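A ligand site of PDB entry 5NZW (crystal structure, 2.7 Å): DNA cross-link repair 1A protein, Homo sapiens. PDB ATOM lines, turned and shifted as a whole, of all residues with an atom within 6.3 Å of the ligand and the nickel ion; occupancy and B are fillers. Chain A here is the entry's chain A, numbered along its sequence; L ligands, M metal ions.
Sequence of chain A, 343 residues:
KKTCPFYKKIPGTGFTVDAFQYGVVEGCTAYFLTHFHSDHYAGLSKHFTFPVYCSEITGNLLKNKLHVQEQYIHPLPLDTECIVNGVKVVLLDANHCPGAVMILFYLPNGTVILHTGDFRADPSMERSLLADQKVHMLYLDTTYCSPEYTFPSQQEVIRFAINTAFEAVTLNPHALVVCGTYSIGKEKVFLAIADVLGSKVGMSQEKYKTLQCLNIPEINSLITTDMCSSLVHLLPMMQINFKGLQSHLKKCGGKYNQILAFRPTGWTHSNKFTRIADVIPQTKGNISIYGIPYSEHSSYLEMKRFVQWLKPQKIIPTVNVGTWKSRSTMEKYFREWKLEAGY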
ATOM      1  N   HIS A  35     -22.266 -29.418  -9.438  1.00  0.00           N
ATOM      2  CA  HIS A  35     -21.938 -28.686 -10.658  1.00  0.00           C
ATOM      3  C   HIS A  35     -20.971 -27.528 -10.414  1.00  0.00           C
ATOM      4  O   HIS A  35     -20.695 -27.173  -9.267  1.00  0.00           O
ATOM      5  CB  HIS A  35     -23.219 -28.205 -11.360  1.00  0.00           C
ATOM      6  CG  HIS A  35     -24.014 -27.188 -10.590  1.00  0.00           C
ATOM      7  ND1 HIS A  35     -24.455 -27.389  -9.297  1.00  0.00           N
ATOM      8  CD2 HIS A  35     -24.511 -25.988 -10.966  1.00  0.00           C
ATOM      9  CE1 HIS A  35     -25.157 -26.347  -8.907  1.00  0.00           C
ATOM     10  NE2 HIS A  35     -25.235 -25.485  -9.912  1.00  0.00           N
ATOM     11  N   HIS A  37     -20.807 -24.102 -10.352  1.00  0.00           N
ATOM     12  CA  HIS A  37     -21.379 -22.766 -10.127  1.00  0.00           C
ATOM     13  C   HIS A  37     -20.759 -22.269  -8.811  1.00  0.00           C
ATOM     14  O   HIS A  37     -20.572 -23.051  -7.882  1.00  0.00           O
ATOM     15  CB  HIS A  37     -22.923 -22.799 -10.067  1.00  0.00           C
ATOM     16  CG  HIS A  37     -23.613 -22.810 -11.402  1.00  0.00           C
ATOM     17  ND1 HIS A  37     -24.964 -23.054 -11.541  1.00  0.00           N
ATOM     18  CD2 HIS A  37     -23.141 -22.608 -12.665  1.00  0.00           C
ATOM     19  CE1 HIS A  37     -25.291 -22.993 -12.827  1.00  0.00           C
ATOM     20  NE2 HIS A  37     -24.209 -22.737 -13.527  1.00  0.00           N
ATOM     21  N   SER A  38     -20.423 -20.976  -8.754  1.00  0.00           N
ATOM     22  CA  SER A  38     -19.527 -20.471  -7.699  1.00  0.00           C
ATOM     23  C   SER A  38     -20.098 -20.450  -6.277  1.00  0.00           C
ATOM     24  O   SER A  38     -19.330 -20.587  -5.329  1.00  0.00           O
ATOM     25  CB  SER A  38     -18.958 -19.085  -8.067  1.00  0.00           C
ATOM     26  OG  SER A  38     -19.912 -18.306  -8.765  1.00  0.00           O
ATOM     27  N   ASP A  39     -21.415 -20.250  -6.142  1.00  0.00           N
ATOM     28  CA  ASP A  39     -22.097 -20.539  -4.875  1.00  0.00           C
ATOM     29  C   ASP A  39     -21.743 -21.952  -4.417  1.00  0.00           C
ATOM     30  O   ASP A  39     -21.469 -22.155  -3.231  1.00  0.00           O
ATOM     31  CB  ASP A  39     -23.629 -20.424  -5.013  1.00  0.00           C
ATOM     32  CG  ASP A  39     -24.180 -19.029  -4.662  1.00  0.00           C
ATOM     33  OD1 ASP A  39     -23.625 -18.015  -5.160  1.00  0.00           O
ATOM     34  OD2 ASP A  39     -25.184 -18.952  -3.912  1.00  0.00           O
ATOM     35  N   HIS A  40     -21.702 -22.883  -5.372  1.00  0.00           N
ATOM     36  CA  HIS A  40     -21.471 -24.326  -5.121  1.00  0.00           C
ATOM     37  C   HIS A  40     -20.029 -24.791  -5.115  1.00  0.00           C
ATOM     38  O   HIS A  40     -19.785 -25.934  -4.733  1.00  0.00           O
ATOM     39  CB  HIS A  40     -22.262 -25.215  -6.113  1.00  0.00           C
ATOM     40  CG  HIS A  40     -23.725 -24.884  -6.164  1.00  0.00           C
ATOM     41  ND1 HIS A  40     -24.658 -25.514  -5.386  1.00  0.00           N
ATOM     42  CD2 HIS A  40     -24.387 -23.939  -6.868  1.00  0.00           C
ATOM     43  CE1 HIS A  40     -25.851 -24.973  -5.604  1.00  0.00           C
ATOM     44  NE2 HIS A  40     -25.718 -24.030  -6.515  1.00  0.00           N
ATOM     45  N   HIS A  96     -29.566 -29.136 -15.778  1.00  0.00           N
ATOM     46  CA  HIS A  96     -29.260 -27.855 -15.196  1.00  0.00           C
ATOM     47  C   HIS A  96     -28.240 -27.215 -16.118  1.00  0.00           C
ATOM     48  O   HIS A  96     -28.627 -26.753 -17.179  1.00  0.00           O
ATOM     49  CB  HIS A  96     -28.781 -28.050 -13.771  1.00  0.00           C
ATOM     50  CG  HIS A  96     -28.483 -26.776 -13.068  1.00  0.00           C
ATOM     51  ND1 HIS A  96     -29.431 -25.782 -12.917  1.00  0.00           N
ATOM     52  CD2 HIS A  96     -27.356 -26.326 -12.477  1.00  0.00           C
ATOM     53  CE1 HIS A  96     -28.902 -24.774 -12.246  1.00  0.00           C
ATOM     54  NE2 HIS A  96     -27.638 -25.082 -11.974  1.00  0.00           N
ATOM     55  N   CYS A  97     -26.968 -27.205 -15.779  1.00  0.00           N
ATOM     56  CA  CYS A  97     -25.982 -26.696 -16.712  1.00  0.00           C
ATOM     57  C   CYS A  97     -25.133 -27.878 -17.125  1.00  0.00           C
ATOM     58  O   CYS A  97     -25.191 -28.898 -16.475  1.00  0.00           O
ATOM     59  CB  CYS A  97     -25.152 -25.621 -16.036  1.00  0.00           C
ATOM     60  SG  CYS A  97     -24.234 -26.258 -14.653  1.00  0.00           S
ATOM     61  N   ASP A 118     -28.410 -28.551  -7.978  1.00  0.00           N
ATOM     62  CA  ASP A 118     -29.275 -27.720  -8.807  1.00  0.00           C
ATOM     63  C   ASP A 118     -29.804 -28.572  -9.960  1.00  0.00           C
ATOM     64  O   ASP A 118     -29.053 -29.346 -10.573  1.00  0.00           O
ATOM     65  CB  ASP A 118     -28.553 -26.487  -9.327  1.00  0.00           C
ATOM     66  CG  ASP A 118     -28.365 -25.417  -8.255  1.00  0.00           C
ATOM     67  OD1 ASP A 118     -28.782 -25.623  -7.077  1.00  0.00           O
ATOM     68  OD2 ASP A 118     -27.801 -24.353  -8.610  1.00  0.00           O
ATOM     69  N   ASP A 141     -33.387 -28.686  -4.506  1.00  0.00           N
ATOM     70  CA  ASP A 141     -33.262 -27.357  -5.091  1.00  0.00           C
ATOM     71  C   ASP A 141     -34.627 -26.645  -5.030  1.00  0.00           C
ATOM     72  O   ASP A 141     -35.532 -26.939  -5.800  1.00  0.00           O
ATOM     73  CB  ASP A 141     -32.788 -27.423  -6.527  1.00  0.00           C
ATOM     74  CG  ASP A 141     -32.507 -26.040  -7.134  1.00  0.00           C
ATOM     75  OD1 ASP A 141     -32.647 -25.020  -6.433  1.00  0.00           O
ATOM     76  OD2 ASP A 141     -32.140 -25.981  -8.331  1.00  0.00           O
ATOM     77  N   THR A 143     -34.869 -23.200  -5.067  1.00  0.00           N
ATOM     78  CA  THR A 143     -34.730 -21.914  -5.735  1.00  0.00           C
ATOM     79  C   THR A 143     -36.030 -21.195  -6.162  1.00  0.00           C
ATOM     80  O   THR A 143     -36.098 -19.968  -6.064  1.00  0.00           O
ATOM     81  CB  THR A 143     -33.865 -22.097  -7.004  1.00  0.00           C
ATOM     82  OG1 THR A 143     -32.583 -22.601  -6.633  1.00  0.00           O
ATOM     83  CG2 THR A 143     -33.687 -20.765  -7.771  1.00  0.00           C
ATOM     84  N   TYR A 144     -37.025 -21.914  -6.658  1.00  0.00           N
ATOM     85  CA  TYR A 144     -38.295 -21.300  -7.061  1.00  0.00           C
ATOM     86  C   TYR A 144     -39.504 -22.001  -6.420  1.00  0.00           C
ATOM     87  O   TYR A 144     -40.584 -22.103  -7.026  1.00  0.00           O
ATOM     88  CB  TYR A 144     -38.438 -21.298  -8.600  1.00  0.00           C
ATOM     89  CG  TYR A 144     -37.460 -20.449  -9.390  1.00  0.00           C
ATOM     90  CD1 TYR A 144     -37.397 -19.064  -9.215  1.00  0.00           C
ATOM     91  CD2 TYR A 144     -36.648 -21.026 -10.357  1.00  0.00           C
ATOM     92  CE1 TYR A 144     -36.522 -18.286  -9.958  1.00  0.00           C
ATOM     93  CE2 TYR A 144     -35.768 -20.254 -11.111  1.00  0.00           C
ATOM     94  CZ  TYR A 144     -35.715 -18.892 -10.922  1.00  0.00           C
ATOM     95  OH  TYR A 144     -34.829 -18.161 -11.696  1.00  0.00           O
ATOM     96  N   TYR A 182     -22.480 -15.157 -18.109  1.00  0.00           N
ATOM     97  CA  TYR A 182     -21.428 -15.033 -17.064  1.00  0.00           C
ATOM     98  C   TYR A 182     -20.745 -16.361 -16.742  1.00  0.00           C
ATOM     99  O   TYR A 182     -19.523 -16.517 -16.944  1.00  0.00           O
ATOM    100  CB  TYR A 182     -21.951 -14.374 -15.760  1.00  0.00           C
ATOM    101  CG  TYR A 182     -23.360 -14.722 -15.307  1.00  0.00           C
ATOM    102  CD1 TYR A 182     -24.474 -14.211 -15.980  1.00  0.00           C
ATOM    103  CD2 TYR A 182     -23.584 -15.523 -14.184  1.00  0.00           C
ATOM    104  CE1 TYR A 182     -25.772 -14.503 -15.562  1.00  0.00           C
ATOM    105  CE2 TYR A 182     -24.881 -15.829 -13.767  1.00  0.00           C
ATOM    106  CZ  TYR A 182     -25.973 -15.307 -14.461  1.00  0.00           C
ATOM    107  OH  TYR A 182     -27.258 -15.588 -14.076  1.00  0.00           O
ATOM    108  N   MET A 238     -22.997  -7.969 -18.090  1.00  0.00           N
ATOM    109  CA  MET A 238     -22.862  -6.534 -17.770  1.00  0.00           C
ATOM    110  C   MET A 238     -22.730  -5.671 -19.028  1.00  0.00           C
ATOM    111  O   MET A 238     -23.263  -4.578 -19.083  1.00  0.00           O
ATOM    112  CB  MET A 238     -21.682  -6.285 -16.812  1.00  0.00           C
ATOM    113  CG  MET A 238     -21.746  -7.080 -15.505  1.00  0.00           C
ATOM    114  SD  MET A 238     -21.722  -6.118 -13.975  1.00  0.00           S
ATOM    115  CE  MET A 238     -23.468  -5.726 -13.761  1.00  0.00           C
ATOM    116  N   THR A 265     -31.967 -14.077 -18.150  1.00  0.00           N
ATOM    117  CA  THR A 265     -32.234 -14.224 -16.715  1.00  0.00           C
ATOM    118  C   THR A 265     -33.736 -14.181 -16.416  1.00  0.00           C
ATOM    119  O   THR A 265     -34.266 -15.075 -15.735  1.00  0.00           O
ATOM    120  CB  THR A 265     -31.470 -13.163 -15.899  1.00  0.00           C
ATOM    121  OG1 THR A 265     -31.361 -11.953 -16.672  1.00  0.00           O
ATOM    122  CG2 THR A 265     -30.054 -13.665 -15.561  1.00  0.00           C
ATOM    123  N   GLY A 266     -34.424 -13.156 -16.931  1.00  0.00           N
ATOM    124  CA  GLY A 266     -35.866 -12.988 -16.718  1.00  0.00           C
ATOM    125  C   GLY A 266     -36.530 -12.103 -17.745  1.00  0.00           C
ATOM    126  O   GLY A 266     -36.246 -12.196 -18.940  1.00  0.00           O
ATOM    127  N   GLU A 296     -32.867 -22.787 -15.768  1.00  0.00           N
ATOM    128  CA  GLU A 296     -32.356 -24.130 -15.615  1.00  0.00           C
ATOM    129  C   GLU A 296     -32.635 -24.583 -14.212  1.00  0.00           C
ATOM    130  O   GLU A 296     -31.856 -25.331 -13.639  1.00  0.00           O
ATOM    131  CB  GLU A 296     -30.863 -24.189 -15.893  1.00  0.00           C
ATOM    132  CG  GLU A 296     -30.502 -23.833 -17.320  1.00  0.00           C
ATOM    133  CD  GLU A 296     -29.000 -23.816 -17.546  1.00  0.00           C
ATOM    134  OE1 GLU A 296     -28.235 -23.440 -16.600  1.00  0.00           O
ATOM    135  OE2 GLU A 296     -28.604 -24.192 -18.682  1.00  0.00           O
ATOM    136  N   HIS A 297     -33.738 -24.099 -13.663  1.00  0.00           N
ATOM    137  CA  HIS A 297     -34.237 -24.514 -12.341  1.00  0.00           C
ATOM    138  C   HIS A 297     -35.721 -24.849 -12.505  1.00  0.00           C
ATOM    139  O   HIS A 297     -36.405 -24.309 -13.376  1.00  0.00           O
ATOM    140  CB  HIS A 297     -34.140 -23.373 -11.322  1.00  0.00           C
ATOM    141  CG  HIS A 297     -32.778 -23.126 -10.725  1.00  0.00           C
ATOM    142  ND1 HIS A 297     -32.292 -23.834  -9.657  1.00  0.00           N
ATOM    143  CD2 HIS A 297     -31.866 -22.159 -10.978  1.00  0.00           C
ATOM    144  CE1 HIS A 297     -31.122 -23.338  -9.292  1.00  0.00           C
ATOM    145  NE2 HIS A 297     -30.844 -22.322 -10.085  1.00  0.00           N
HETATM  146  C1  LIG L   1     -29.889 -14.181 -11.990  1.00  0.00           C
HETATM  147  S1  LIG L   1     -28.297 -14.392 -11.182  1.00  0.00           S
HETATM  148  C2  LIG L   1     -28.808 -15.676 -10.003  1.00  0.00           C
HETATM  149  C3  LIG L   1     -30.157 -16.351 -10.199  1.00  0.00           C
HETATM  150  C4  LIG L   1     -30.133 -17.866 -10.068  1.00  0.00           C
HETATM  151  S2  LIG L   1     -29.769 -18.402  -8.371  1.00  0.00           S
HETATM  152  C5  LIG L   1     -28.513 -19.610  -8.551  1.00  0.00           C
HETATM  153  N1  LIG L   1     -28.606 -20.564  -9.482  1.00  0.00           N
HETATM  154  C6  LIG L   1     -27.595 -21.497  -9.573  1.00  0.00           C
HETATM  155  O1  LIG L   1     -27.729 -22.366 -10.454  1.00  0.00           O
HETATM  156  C7  LIG L   1     -26.511 -21.473  -8.729  1.00  0.00           C
HETATM  157  O2  LIG L   1     -25.633 -22.307  -8.821  1.00  0.00           O
HETATM  158  N2  LIG L   1     -26.408 -20.513  -7.762  1.00  0.00           N
HETATM  159  N3  LIG L   1     -27.451 -19.547  -7.677  1.00  0.00           N
HETATM  160  C8  LIG L   1     -27.340 -18.512  -6.641  1.00  0.00           C
HETATM  161  C9  LIG L   1     -31.267 -15.590 -10.386  1.00  0.00           C
HETATM  162  N4  LIG L   1     -30.995 -14.404 -11.052  1.00  0.00           N
HETATM  163  C10 LIG L   1     -31.569 -13.159 -11.100  1.00  0.00           C
HETATM  164  O3  LIG L   1     -32.509 -12.673 -10.535  1.00  0.00           O
HETATM  165  C11 LIG L   1     -30.509 -12.701 -12.136  1.00  0.00           C
HETATM  166  N5  LIG L   1     -29.678 -11.551 -11.883  1.00  0.00           N
HETATM  167  C12 LIG L   1     -29.296 -11.074 -10.670  1.00  0.00           C
HETATM  168  O4  LIG L   1     -29.655 -11.594  -9.607  1.00  0.00           O
HETATM  169  C13 LIG L   1     -28.356  -9.902 -10.601  1.00  0.00           C
HETATM  170  N6  LIG L   1     -27.213 -10.003 -11.170  1.00  0.00           N
HETATM  171  O5  LIG L   1     -26.167  -9.495 -10.372  1.00  0.00           O
HETATM  172  C14 LIG L   1     -25.576  -8.356 -10.993  1.00  0.00           C
HETATM  173  C15 LIG L   1     -28.791  -8.630  -9.995  1.00  0.00           C
HETATM  174  C16 LIG L   1     -28.125  -7.937  -9.041  1.00  0.00           C
HETATM  175  S3  LIG L   1     -28.817  -6.384  -8.844  1.00  0.00           S
HETATM  176  C17 LIG L   1     -29.974  -6.792 -10.089  1.00  0.00           C
HETATM  177  N7  LIG L   1     -30.753  -5.853 -10.655  1.00  0.00           N
HETATM  178  N8  LIG L   1     -29.990  -8.065 -10.409  1.00  0.00           N
HETATM  179  C18 LIG L   1     -32.684 -15.933  -9.903  1.00  0.00           C
HETATM  180  O6  LIG L   1     -33.613 -15.347 -10.432  1.00  0.00           O
HETATM  181  O7  LIG L   1     -32.792 -16.752  -9.000  1.00  0.00           O
HETATM  182 NI    NI M   1     -26.522 -23.860 -10.454  1.00  0.00          NI
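O1 of the ligand binds the nickel ion, 1.9 Å away. ND1 of His 37 is bound to the nickel ion. NE2 of His 35 is bound to the nickel ion. NE2 of His 96 binds the nickel ion (2.2 Å). OD2 of Asp 118 binds the nickel ion (2.3 Å). O2 of the ligand binds the nickel ion (2.4 Å). The nickel ion has six donor atoms within binding distance.
A ring nitrogen (ND1) of His 297 sits close to the side-chain hydroxyl of Thr 143. The backbone carbonyl oxygen of Glu 296 is in hydrogen-bond range of a ring nitrogen (ND1) of His 96, at 2.6 Å. The side-chain carboxylate (OD1) of Asp 118 sits close to a ring nitrogen (NE2) of His 40 (3.5 Å). NE2 of His 37 is in hydrogen-bond range of SG of Cys 97. ND1 of His 297 is in hydrogen-bond range of OD2 of Asp 141 (2.5 Å).
An oxygen (O2) of the ligand sits close to a ring nitrogen (NE2) of His 40. The side-chain hydroxyl (OH) of Tyr 144 is in hydrogen-bond range of an oxygen (O6) of the ligand. A sulfur (S1) of the ligand sits close to the side-chain hydroxyl (OH) of Tyr 182, at 3.3 Å. NE2 of His 297 lies within hydrogen-bond range of N1 of the ligand, at 2.9 Å.
The nearest printed residue that does not touch the nickel ion is His 40 (4.02 Å).
Asp 39 touches the ligand. Thr 265 touches the ligand. Of the 17 residues printed, 10 come within 4 Å of the ligand. The nearest printed residue that does not touch the ligand is Thr 143 (4.3 Å).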
